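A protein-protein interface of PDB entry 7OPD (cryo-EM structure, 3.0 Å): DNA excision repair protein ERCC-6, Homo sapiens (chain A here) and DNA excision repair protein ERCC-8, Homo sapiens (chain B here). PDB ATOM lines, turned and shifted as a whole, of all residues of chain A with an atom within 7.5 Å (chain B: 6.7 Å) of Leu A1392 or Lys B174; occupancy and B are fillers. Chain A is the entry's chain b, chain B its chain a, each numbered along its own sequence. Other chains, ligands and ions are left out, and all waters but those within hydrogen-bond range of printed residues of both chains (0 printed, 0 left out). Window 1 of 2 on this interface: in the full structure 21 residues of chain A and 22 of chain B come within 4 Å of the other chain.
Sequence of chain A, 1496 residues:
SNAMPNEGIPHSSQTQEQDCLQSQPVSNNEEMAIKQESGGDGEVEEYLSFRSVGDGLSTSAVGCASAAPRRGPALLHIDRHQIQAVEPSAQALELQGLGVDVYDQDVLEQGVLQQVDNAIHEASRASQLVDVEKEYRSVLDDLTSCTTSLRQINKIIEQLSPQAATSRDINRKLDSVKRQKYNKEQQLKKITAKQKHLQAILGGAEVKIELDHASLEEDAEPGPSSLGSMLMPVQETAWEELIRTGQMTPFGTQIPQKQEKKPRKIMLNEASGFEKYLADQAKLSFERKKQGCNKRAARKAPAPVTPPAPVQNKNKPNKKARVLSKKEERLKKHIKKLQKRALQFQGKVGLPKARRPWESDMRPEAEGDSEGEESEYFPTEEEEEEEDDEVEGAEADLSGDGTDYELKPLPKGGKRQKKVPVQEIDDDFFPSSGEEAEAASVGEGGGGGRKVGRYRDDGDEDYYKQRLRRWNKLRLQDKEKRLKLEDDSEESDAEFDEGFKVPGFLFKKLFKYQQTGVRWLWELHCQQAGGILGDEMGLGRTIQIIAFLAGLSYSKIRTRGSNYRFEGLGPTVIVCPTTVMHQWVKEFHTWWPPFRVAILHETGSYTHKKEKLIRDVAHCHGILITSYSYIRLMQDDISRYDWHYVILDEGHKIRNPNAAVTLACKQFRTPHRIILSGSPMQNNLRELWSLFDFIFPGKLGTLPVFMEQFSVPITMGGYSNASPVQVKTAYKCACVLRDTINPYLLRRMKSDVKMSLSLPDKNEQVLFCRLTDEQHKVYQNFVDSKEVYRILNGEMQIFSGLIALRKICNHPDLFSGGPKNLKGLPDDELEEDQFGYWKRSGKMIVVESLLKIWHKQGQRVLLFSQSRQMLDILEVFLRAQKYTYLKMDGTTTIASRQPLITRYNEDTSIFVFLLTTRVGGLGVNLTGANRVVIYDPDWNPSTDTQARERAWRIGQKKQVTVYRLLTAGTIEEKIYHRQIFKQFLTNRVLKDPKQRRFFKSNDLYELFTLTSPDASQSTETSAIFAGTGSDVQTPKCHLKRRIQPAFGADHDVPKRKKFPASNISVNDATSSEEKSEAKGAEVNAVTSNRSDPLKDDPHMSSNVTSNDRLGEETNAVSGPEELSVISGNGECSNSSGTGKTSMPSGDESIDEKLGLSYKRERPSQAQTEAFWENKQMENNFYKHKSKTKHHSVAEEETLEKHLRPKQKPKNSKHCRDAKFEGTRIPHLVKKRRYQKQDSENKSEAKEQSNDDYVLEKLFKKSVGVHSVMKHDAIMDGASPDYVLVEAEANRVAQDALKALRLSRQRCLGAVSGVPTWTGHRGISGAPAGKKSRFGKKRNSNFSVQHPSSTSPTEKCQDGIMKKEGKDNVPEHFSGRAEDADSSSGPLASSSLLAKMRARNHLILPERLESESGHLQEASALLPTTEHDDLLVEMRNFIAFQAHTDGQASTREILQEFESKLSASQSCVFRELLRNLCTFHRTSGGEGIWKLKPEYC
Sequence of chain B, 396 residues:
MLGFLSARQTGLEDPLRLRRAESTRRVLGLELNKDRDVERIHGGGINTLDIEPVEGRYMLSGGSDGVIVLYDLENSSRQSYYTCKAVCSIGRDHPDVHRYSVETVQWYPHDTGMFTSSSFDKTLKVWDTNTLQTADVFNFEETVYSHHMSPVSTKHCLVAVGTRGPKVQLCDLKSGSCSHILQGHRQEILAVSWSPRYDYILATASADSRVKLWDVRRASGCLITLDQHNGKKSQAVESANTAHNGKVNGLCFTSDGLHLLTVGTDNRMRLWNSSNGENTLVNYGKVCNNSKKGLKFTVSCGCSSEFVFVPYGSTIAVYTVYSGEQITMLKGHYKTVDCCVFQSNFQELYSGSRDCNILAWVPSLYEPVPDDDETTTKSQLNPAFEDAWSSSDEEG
The side-chain hydroxyl (OH) of Tyr B108 sits at hydrogen-bond distance from the backbone carbonyl oxygen (O) of Leu A1387 (2.7 Å). O of Leu B173 is in hydrogen-bond range of NH2 of Arg A1399 (3.2 Å). The side-chain carboxylate (OD2) of Asp A739 is in hydrogen-bond range of the side-chain hydroxyl (OG) of Ser B175 (2.5 Å). NE of Arg A1399 sits close to N of Gly B176 (3.3 Å).
The backbone NH of Tyr B108 sits close to the backbone carbonyl oxygen of Met B114, at 2.9 Å. The backbone NH (N) of Leu B173 lies within hydrogen-bond range of the backbone carbonyl oxygen (O) of Cys B157 (3.2 Å). The side-chain carboxylate of Asp B172 sits at hydrogen-bond distance from the backbone NH of Lys B174, 3.2 Å away.
Printed residues of chain B that touch a printed residue of chain A: Tyr B108, Met B114, Ala B135, Leu B173, Lys B174, Ser B175 and Gly B176. Hydrophobic or aromatic side chains of chain B within 4 Å of the printed part of chain A: Tyr B108, Met B114, Ala B135 and Leu B173. Of the 15 printed residues of chain A, 7 touch a printed residue of chain B. Hydrophobic or aromatic side chains of chain A within 4 Å of the printed part of chain B: Leu A1392, Leu A1393 and Met A1396. Along chain A the printed residues that touch a printed residue of chain B span positions 739 to 1399. Among the printed residues, no Asp or Glu carboxylate lies within 4 Å of a Lys or Arg side-chain nitrogen of the other chain.
Of chain B, only Tyr B108 (3.8 Å), Met B114 (3.9 Å) and Lys B174 (3.8 Å) come within 4 Å of Leu A1392. Printed residues of chain A within 4 Å of Lys B174: Leu A1392. Of the printed residues of chain B, Asp A739 touches Ser B175 (2.5 Å). Of the printed residues of chain B, Arg A1399 touches Leu B173 (3.2 Å), Ser B175 (3.7 Å) and Gly B176 (3.3 Å). Printed residues of chain A within 4 Å of Leu B173: Met A1396 (3.3 Å) and Arg A1399 (3.2 Å). The nearest printed residue of chain B that does not touch Leu A1392 is Cys B157 (4.2 Å). The nearest residue of chain A that does not touch Lys B174 is Arg A1399 (4.5 Å).
Among the printed residues, pairs that only touch across the chains: Leu A1393 with Ala B135 (3.3 Å), Met A1396 with Leu B173 (3.3 Å), Met A1396 with Ala B135 (3.4 Å), Ser A1389 with Tyr B108 (3.7 Å), Arg A1399 with Ser B175 (3.7 Å), Leu A1393 with Met B114 (3.7 Å), Leu A1392 with Lys B174 (3.8 Å), Leu A1392 with Tyr B108 (3.8 Å) and Leu A1392 with Met B114 (3.9 Å).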
ATOM      1  N   ASP A 739      -9.834   0.019  -9.720  1.00  0.00           N
ATOM      2  CA  ASP A 739      -9.819  -0.150 -11.152  1.00  0.00           C
ATOM      3  C   ASP A 739      -8.798  -1.169 -11.555  1.00  0.00           C
ATOM      4  O   ASP A 739      -9.031  -1.962 -12.450  1.00  0.00           O
ATOM      5  CB  ASP A 739      -9.573   1.189 -11.812  1.00  0.00           C
ATOM      6  CG  ASP A 739     -10.726   2.143 -11.593  1.00  0.00           C
ATOM      7  OD1 ASP A 739     -11.875   1.660 -11.509  1.00  0.00           O
ATOM      8  OD2 ASP A 739     -10.517   3.368 -11.518  1.00  0.00           O
ATOM      9  N   PRO A1386     -13.102   2.897 -29.482  1.00  0.00           N
ATOM     10  CA  PRO A1386     -11.979   3.520 -28.787  1.00  0.00           C
ATOM     11  C   PRO A1386     -12.368   4.779 -28.053  1.00  0.00           C
ATOM     12  O   PRO A1386     -13.100   5.598 -28.578  1.00  0.00           O
ATOM     13  CB  PRO A1386     -11.006   3.830 -29.914  1.00  0.00           C
ATOM     14  CG  PRO A1386     -11.824   3.970 -31.103  1.00  0.00           C
ATOM     15  CD  PRO A1386     -13.020   3.099 -30.935  1.00  0.00           C
ATOM     16  N   LEU A1387     -11.879   4.923 -26.833  1.00  0.00           N
ATOM     17  CA  LEU A1387     -12.125   6.139 -26.091  1.00  0.00           C
ATOM     18  C   LEU A1387     -11.557   7.296 -26.865  1.00  0.00           C
ATOM     19  O   LEU A1387     -10.426   7.244 -27.338  1.00  0.00           O
ATOM     20  CB  LEU A1387     -11.481   6.078 -24.719  1.00  0.00           C
ATOM     21  CG  LEU A1387     -12.211   5.339 -23.607  1.00  0.00           C
ATOM     22  CD1 LEU A1387     -13.507   6.023 -23.242  1.00  0.00           C
ATOM     23  CD2 LEU A1387     -12.474   3.908 -23.986  1.00  0.00           C
ATOM     24  N   ALA A1388     -12.351   8.327 -27.024  1.00  0.00           N
ATOM     25  CA  ALA A1388     -11.978   9.379 -27.936  1.00  0.00           C
ATOM     26  C   ALA A1388     -11.269  10.500 -27.227  1.00  0.00           C
ATOM     27  O   ALA A1388     -11.671  11.640 -27.347  1.00  0.00           O
ATOM     28  CB  ALA A1388     -13.215   9.898 -28.645  1.00  0.00           C
ATOM     29  N   SER A1389     -10.278  10.205 -26.416  1.00  0.00           N
ATOM     30  CA  SER A1389      -9.275  11.179 -25.987  1.00  0.00           C
ATOM     31  C   SER A1389      -9.857  12.440 -25.412  1.00  0.00           C
ATOM     32  O   SER A1389      -9.165  13.426 -25.285  1.00  0.00           O
ATOM     33  CB  SER A1389      -8.373  11.599 -27.128  1.00  0.00           C
ATOM     34  OG  SER A1389      -9.031  12.619 -27.828  1.00  0.00           O
ATOM     35  N   SER A1390     -11.057  12.464 -25.125  1.00  0.00           N
ATOM     36  CA  SER A1390     -11.664  13.502 -24.353  1.00  0.00           C
ATOM     37  C   SER A1390     -12.395  12.872 -23.212  1.00  0.00           C
ATOM     38  O   SER A1390     -12.416  13.408 -22.122  1.00  0.00           O
ATOM     39  CB  SER A1390     -12.595  14.275 -25.191  1.00  0.00           C
ATOM     40  OG  SER A1390     -11.919  14.736 -26.324  1.00  0.00           O
ATOM     41  N   SER A1391     -12.980  11.718 -23.441  1.00  0.00           N
ATOM     42  CA  SER A1391     -13.342  10.895 -22.324  1.00  0.00           C
ATOM     43  C   SER A1391     -12.116  10.564 -21.515  1.00  0.00           C
ATOM     44  O   SER A1391     -12.133  10.667 -20.288  1.00  0.00           O
ATOM     45  CB  SER A1391     -13.998   9.642 -22.826  1.00  0.00           C
ATOM     46  OG  SER A1391     -13.191   9.137 -23.846  1.00  0.00           O
ATOM     47  N   LEU A1392     -11.032  10.194 -22.171  1.00  0.00           N
ATOM     48  CA  LEU A1392      -9.820   9.965 -21.419  1.00  0.00           C
ATOM     49  C   LEU A1392      -9.413  11.203 -20.693  1.00  0.00           C
ATOM     50  O   LEU A1392      -9.218  11.170 -19.489  1.00  0.00           O
ATOM     51  CB  LEU A1392      -8.686   9.556 -22.316  1.00  0.00           C
ATOM     52  CG  LEU A1392      -8.623   8.104 -22.724  1.00  0.00           C
ATOM     53  CD1 LEU A1392      -7.416   7.969 -23.555  1.00  0.00           C
ATOM     54  CD2 LEU A1392      -8.552   7.124 -21.616  1.00  0.00           C
ATOM     55  N   LEU A1393      -9.286  12.305 -21.388  1.00  0.00           N
ATOM     56  CA  LEU A1393      -8.712  13.446 -20.721  1.00  0.00           C
ATOM     57  C   LEU A1393      -9.641  13.961 -19.670  1.00  0.00           C
ATOM     58  O   LEU A1393      -9.202  14.508 -18.669  1.00  0.00           O
ATOM     59  CB  LEU A1393      -8.392  14.535 -21.693  1.00  0.00           C
ATOM     60  CG  LEU A1393      -7.295  14.221 -22.651  1.00  0.00           C
ATOM     61  CD1 LEU A1393      -7.284  15.277 -23.590  1.00  0.00           C
ATOM     62  CD2 LEU A1393      -6.005  14.212 -22.009  1.00  0.00           C
ATOM     63  N   ALA A1394     -10.932  13.834 -19.885  1.00  0.00           N
ATOM     64  CA  ALA A1394     -11.841  14.216 -18.833  1.00  0.00           C
ATOM     65  C   ALA A1394     -11.619  13.356 -17.615  1.00  0.00           C
ATOM     66  O   ALA A1394     -11.547  13.862 -16.497  1.00  0.00           O
ATOM     67  CB  ALA A1394     -13.267  14.092 -19.324  1.00  0.00           C
ATOM     68  N   LYS A1395     -11.479  12.055 -17.812  1.00  0.00           N
ATOM     69  CA  LYS A1395     -11.264  11.178 -16.684  1.00  0.00           C
ATOM     70  C   LYS A1395      -9.965  11.502 -15.992  1.00  0.00           C
ATOM     71  O   LYS A1395      -9.883  11.507 -14.765  1.00  0.00           O
ATOM     72  CB  LYS A1395     -11.283   9.742 -17.150  1.00  0.00           C
ATOM     73  CG  LYS A1395     -12.658   9.287 -17.424  1.00  0.00           C
ATOM     74  CD  LYS A1395     -12.718   7.859 -17.883  1.00  0.00           C
ATOM     75  CE  LYS A1395     -14.156   7.408 -17.950  1.00  0.00           C
ATOM     76  NZ  LYS A1395     -14.350   6.000 -18.296  1.00  0.00           N
ATOM     77  N   MET A1396      -8.943  11.785 -16.760  1.00  0.00           N
ATOM     78  CA  MET A1396      -7.676  12.146 -16.170  1.00  0.00           C
ATOM     79  C   MET A1396      -7.808  13.413 -15.365  1.00  0.00           C
ATOM     80  O   MET A1396      -7.281  13.515 -14.260  1.00  0.00           O
ATOM     81  CB  MET A1396      -6.632  12.340 -17.246  1.00  0.00           C
ATOM     82  CG  MET A1396      -5.966  11.108 -17.641  1.00  0.00           C
ATOM     83  SD  MET A1396      -5.272  11.242 -19.255  1.00  0.00           S
ATOM     84  CE  MET A1396      -5.088   9.544 -19.600  1.00  0.00           C
ATOM     85  N   ARG A1397      -8.471  14.408 -15.913  1.00  0.00           N
ATOM     86  CA  ARG A1397      -8.594  15.644 -15.177  1.00  0.00           C
ATOM     87  C   ARG A1397      -9.375  15.427 -13.909  1.00  0.00           C
ATOM     88  O   ARG A1397      -9.068  16.017 -12.878  1.00  0.00           O
ATOM     89  CB  ARG A1397      -9.243  16.698 -16.045  1.00  0.00           C
ATOM     90  CG  ARG A1397      -8.320  17.139 -17.126  1.00  0.00           C
ATOM     91  CD  ARG A1397      -8.733  18.426 -17.761  1.00  0.00           C
ATOM     92  NE  ARG A1397      -7.965  18.683 -18.973  1.00  0.00           N
ATOM     93  CZ  ARG A1397      -6.663  18.961 -19.005  1.00  0.00           C
ATOM     94  NH1 ARG A1397      -5.951  19.049 -17.895  1.00  0.00           N
ATOM     95  NH2 ARG A1397      -6.072  19.177 -20.166  1.00  0.00           N
ATOM     96  N   ALA A1398     -10.361  14.555 -13.953  1.00  0.00           N
ATOM     97  CA  ALA A1398     -11.111  14.271 -12.749  1.00  0.00           C
ATOM     98  C   ALA A1398     -10.205  13.689 -11.689  1.00  0.00           C
ATOM     99  O   ALA A1398     -10.099  14.225 -10.587  1.00  0.00           O
ATOM    100  CB  ALA A1398     -12.247  13.311 -13.063  1.00  0.00           C
ATOM    101  N   ARG A1399      -9.478  12.640 -12.033  1.00  0.00           N
ATOM    102  CA  ARG A1399      -8.636  12.002 -11.040  1.00  0.00           C
ATOM    103  C   ARG A1399      -7.602  12.958 -10.496  1.00  0.00           C
ATOM    104  O   ARG A1399      -7.339  12.966  -9.301  1.00  0.00           O
ATOM    105  CB  ARG A1399      -7.934  10.814 -11.643  1.00  0.00           C
ATOM    106  CG  ARG A1399      -8.700   9.578 -11.554  1.00  0.00           C
ATOM    107  CD  ARG A1399      -7.851   8.402 -11.846  1.00  0.00           C
ATOM    108  NE  ARG A1399      -7.663   8.214 -13.272  1.00  0.00           N
ATOM    109  CZ  ARG A1399      -6.695   8.753 -13.990  1.00  0.00           C
ATOM    110  NH1 ARG A1399      -5.792   9.536 -13.429  1.00  0.00           N
ATOM    111  NH2 ARG A1399      -6.632   8.495 -15.285  1.00  0.00           N
ATOM    112  N   TYR B 108      -1.503   9.817 -29.483  1.00  0.00           N
ATOM    113  CA  TYR B 108      -2.438   8.832 -29.116  1.00  0.00           C
ATOM    114  C   TYR B 108      -2.995   8.288 -30.396  1.00  0.00           C
ATOM    115  O   TYR B 108      -3.558   9.047 -31.171  1.00  0.00           O
ATOM    116  CB  TYR B 108      -3.535   9.448 -28.330  1.00  0.00           C
ATOM    117  CG  TYR B 108      -4.706   8.603 -28.014  1.00  0.00           C
ATOM    118  CD1 TYR B 108      -4.566   7.449 -27.361  1.00  0.00           C
ATOM    119  CD2 TYR B 108      -5.953   9.040 -28.271  1.00  0.00           C
ATOM    120  CE1 TYR B 108      -5.610   6.716 -27.026  1.00  0.00           C
ATOM    121  CE2 TYR B 108      -7.018   8.313 -27.964  1.00  0.00           C
ATOM    122  CZ  TYR B 108      -6.849   7.152 -27.328  1.00  0.00           C
ATOM    123  OH  TYR B 108      -7.923   6.401 -26.991  1.00  0.00           O
ATOM    124  N   MET B 114      -4.658  14.079 -28.037  1.00  0.00           N
ATOM    125  CA  MET B 114      -3.849  13.770 -26.892  1.00  0.00           C
ATOM    126  C   MET B 114      -2.583  13.092 -27.352  1.00  0.00           C
ATOM    127  O   MET B 114      -2.639  12.165 -28.139  1.00  0.00           O
ATOM    128  CB  MET B 114      -4.698  12.904 -25.999  1.00  0.00           C
ATOM    129  CG  MET B 114      -4.120  12.464 -24.709  1.00  0.00           C
ATOM    130  SD  MET B 114      -3.073  11.030 -24.762  1.00  0.00           S
ATOM    131  CE  MET B 114      -4.276   9.779 -24.977  1.00  0.00           C
ATOM    132  N   ALA B 135      -2.426  16.308 -18.897  1.00  0.00           N
ATOM    133  CA  ALA B 135      -3.561  15.714 -18.235  1.00  0.00           C
ATOM    134  C   ALA B 135      -3.171  14.710 -17.199  1.00  0.00           C
ATOM    135  O   ALA B 135      -3.996  14.346 -16.377  1.00  0.00           O
ATOM    136  CB  ALA B 135      -4.458  15.020 -19.224  1.00  0.00           C
ATOM    137  N   PHE B 138       2.877  10.352 -15.018  1.00  0.00           N
ATOM    138  CA  PHE B 138       3.265   9.125 -14.383  1.00  0.00           C
ATOM    139  C   PHE B 138       4.707   9.335 -14.056  1.00  0.00           C
ATOM    140  O   PHE B 138       5.442   9.918 -14.839  1.00  0.00           O
ATOM    141  CB  PHE B 138       3.092   7.936 -15.265  1.00  0.00           C
ATOM    142  CG  PHE B 138       1.738   7.675 -15.616  1.00  0.00           C
ATOM    143  CD1 PHE B 138       1.148   8.352 -16.602  1.00  0.00           C
ATOM    144  CD2 PHE B 138       1.074   6.696 -15.005  1.00  0.00           C
ATOM    145  CE1 PHE B 138      -0.073   8.093 -16.925  1.00  0.00           C
ATOM    146  CE2 PHE B 138      -0.150   6.426 -15.332  1.00  0.00           C
ATOM    147  CZ  PHE B 138      -0.734   7.121 -16.297  1.00  0.00           C
ATOM    148  N   LYS B 155      -9.465  -1.373 -27.251  1.00  0.00           N
ATOM    149  CA  LYS B 155      -9.970  -1.878 -25.986  1.00  0.00           C
ATOM    150  C   LYS B 155      -9.162  -1.397 -24.793  1.00  0.00           C
ATOM    151  O   LYS B 155      -9.725  -0.834 -23.858  1.00  0.00           O
ATOM    152  CB  LYS B 155      -9.989  -3.405 -26.020  1.00  0.00           C
ATOM    153  N   HIS B 156      -7.858  -1.626 -24.799  1.00  0.00           N
ATOM    154  CA  HIS B 156      -6.995  -1.230 -23.704  1.00  0.00           C
ATOM    155  C   HIS B 156      -6.280   0.039 -24.084  1.00  0.00           C
ATOM    156  O   HIS B 156      -6.156   0.361 -25.259  1.00  0.00           O
ATOM    157  CB  HIS B 156      -5.970  -2.299 -23.364  1.00  0.00           C
ATOM    158  CG  HIS B 156      -4.805  -2.382 -24.307  1.00  0.00           C
ATOM    159  ND1 HIS B 156      -3.788  -1.468 -24.326  1.00  0.00           N
ATOM    160  CD2 HIS B 156      -4.435  -3.340 -25.175  1.00  0.00           C
ATOM    161  CE1 HIS B 156      -2.880  -1.818 -25.207  1.00  0.00           C
ATOM    162  NE2 HIS B 156      -3.246  -2.961 -25.729  1.00  0.00           N
ATOM    163  N   CYS B 157      -5.840   0.773 -23.090  1.00  0.00           N
ATOM    164  CA  CYS B 157      -5.059   1.954 -23.384  1.00  0.00           C
ATOM    165  C   CYS B 157      -3.811   1.996 -22.552  1.00  0.00           C
ATOM    166  O   CYS B 157      -3.512   2.988 -21.908  1.00  0.00           O
ATOM    167  CB  CYS B 157      -5.870   3.194 -23.184  1.00  0.00           C
ATOM    168  SG  CYS B 157      -5.183   4.485 -24.157  1.00  0.00           S
ATOM    169  N   LEU B 158      -3.094   0.904 -22.565  1.00  0.00           N
ATOM    170  CA  LEU B 158      -1.872   0.764 -21.841  1.00  0.00           C
ATOM    171  C   LEU B 158      -0.754   1.420 -22.596  1.00  0.00           C
ATOM    172  O   LEU B 158      -0.762   1.444 -23.812  1.00  0.00           O
ATOM    173  CB  LEU B 158      -1.577  -0.679 -21.695  1.00  0.00           C
ATOM    174  CG  LEU B 158      -2.613  -1.382 -20.911  1.00  0.00           C
ATOM    175  CD1 LEU B 158      -2.352  -2.763 -21.118  1.00  0.00           C
ATOM    176  CD2 LEU B 158      -2.539  -1.081 -19.513  1.00  0.00           C
ATOM    177  N   CYS B 171       1.340   1.400 -18.097  1.00  0.00           N
ATOM    178  CA  CYS B 171       0.610   2.509 -17.530  1.00  0.00           C
ATOM    179  C   CYS B 171      -0.733   2.596 -18.189  1.00  0.00           C
ATOM    180  O   CYS B 171      -0.822   2.913 -19.354  1.00  0.00           O
ATOM    181  CB  CYS B 171       1.352   3.802 -17.754  1.00  0.00           C
ATOM    182  SG  CYS B 171       3.001   3.685 -17.335  1.00  0.00           S
ATOM    183  N   ASP B 172      -1.772   2.405 -17.433  1.00  0.00           N
ATOM    184  CA  ASP B 172      -3.109   2.442 -17.975  1.00  0.00           C
ATOM    185  C   ASP B 172      -3.644   3.856 -17.910  1.00  0.00           C
ATOM    186  O   ASP B 172      -3.773   4.417 -16.841  1.00  0.00           O
ATOM    187  CB  ASP B 172      -3.987   1.492 -17.210  1.00  0.00           C
ATOM    188  CG  ASP B 172      -5.138   1.113 -17.979  1.00  0.00           C
ATOM    189  OD1 ASP B 172      -5.798   2.041 -18.462  1.00  0.00           O
ATOM    190  OD2 ASP B 172      -5.381  -0.093 -18.154  1.00  0.00           O
ATOM    191  N   LEU B 173      -3.910   4.447 -19.056  1.00  0.00           N
ATOM    192  CA  LEU B 173      -4.368   5.819 -19.101  1.00  0.00           C
ATOM    193  C   LEU B 173      -5.810   5.941 -18.662  1.00  0.00           C
ATOM    194  O   LEU B 173      -6.176   6.880 -17.966  1.00  0.00           O
ATOM    195  CB  LEU B 173      -4.196   6.326 -20.503  1.00  0.00           C
ATOM    196  CG  LEU B 173      -2.771   6.429 -20.965  1.00  0.00           C
ATOM    197  CD1 LEU B 173      -2.759   6.867 -22.348  1.00  0.00           C
ATOM    198  CD2 LEU B 173      -2.032   7.377 -20.184  1.00  0.00           C
ATOM    199  N   LYS B 174      -6.661   5.021 -19.091  1.00  0.00           N
ATOM    200  CA  LYS B 174      -7.910   4.765 -18.393  1.00  0.00           C
ATOM    201  C   LYS B 174      -7.466   4.445 -16.997  1.00  0.00           C
ATOM    202  O   LYS B 174      -6.323   4.035 -16.842  1.00  0.00           O
ATOM    203  CB  LYS B 174      -8.671   3.599 -19.010  1.00  0.00           C
ATOM    204  N   SER B 175      -8.342   4.461 -16.013  1.00  0.00           N
ATOM    205  CA  SER B 175      -7.950   4.851 -14.667  1.00  0.00           C
ATOM    206  C   SER B 175      -6.531   4.517 -14.286  1.00  0.00           C
ATOM    207  O   SER B 175      -6.124   3.363 -14.289  1.00  0.00           O
ATOM    208  CB  SER B 175      -8.852   4.183 -13.652  1.00  0.00           C
ATOM    209  OG  SER B 175      -8.456   4.538 -12.339  1.00  0.00           O
ATOM    210  N   GLY B 176      -5.814   5.554 -13.910  1.00  0.00           N
ATOM    211  CA  GLY B 176      -4.384   5.613 -13.994  1.00  0.00           C
ATOM    212  C   GLY B 176      -3.678   4.661 -13.095  1.00  0.00           C
ATOM    213  O   GLY B 176      -3.431   4.979 -11.940  1.00  0.00           O
ATOM    214  N   SER B 177      -3.218   3.558 -13.633  1.00  0.00           N
ATOM    215  CA  SER B 177      -2.726   2.473 -12.818  1.00  0.00           C
ATOM    216  C   SER B 177      -1.362   2.079 -13.307  1.00  0.00           C
ATOM    217  O   SER B 177      -1.243   1.183 -14.127  1.00  0.00           O
ATOM    218  CB  SER B 177      -3.651   1.315 -12.910  1.00  0.00           C
ATOM    219  OG  SER B 177      -3.089   0.240 -12.236  1.00  0.00           O
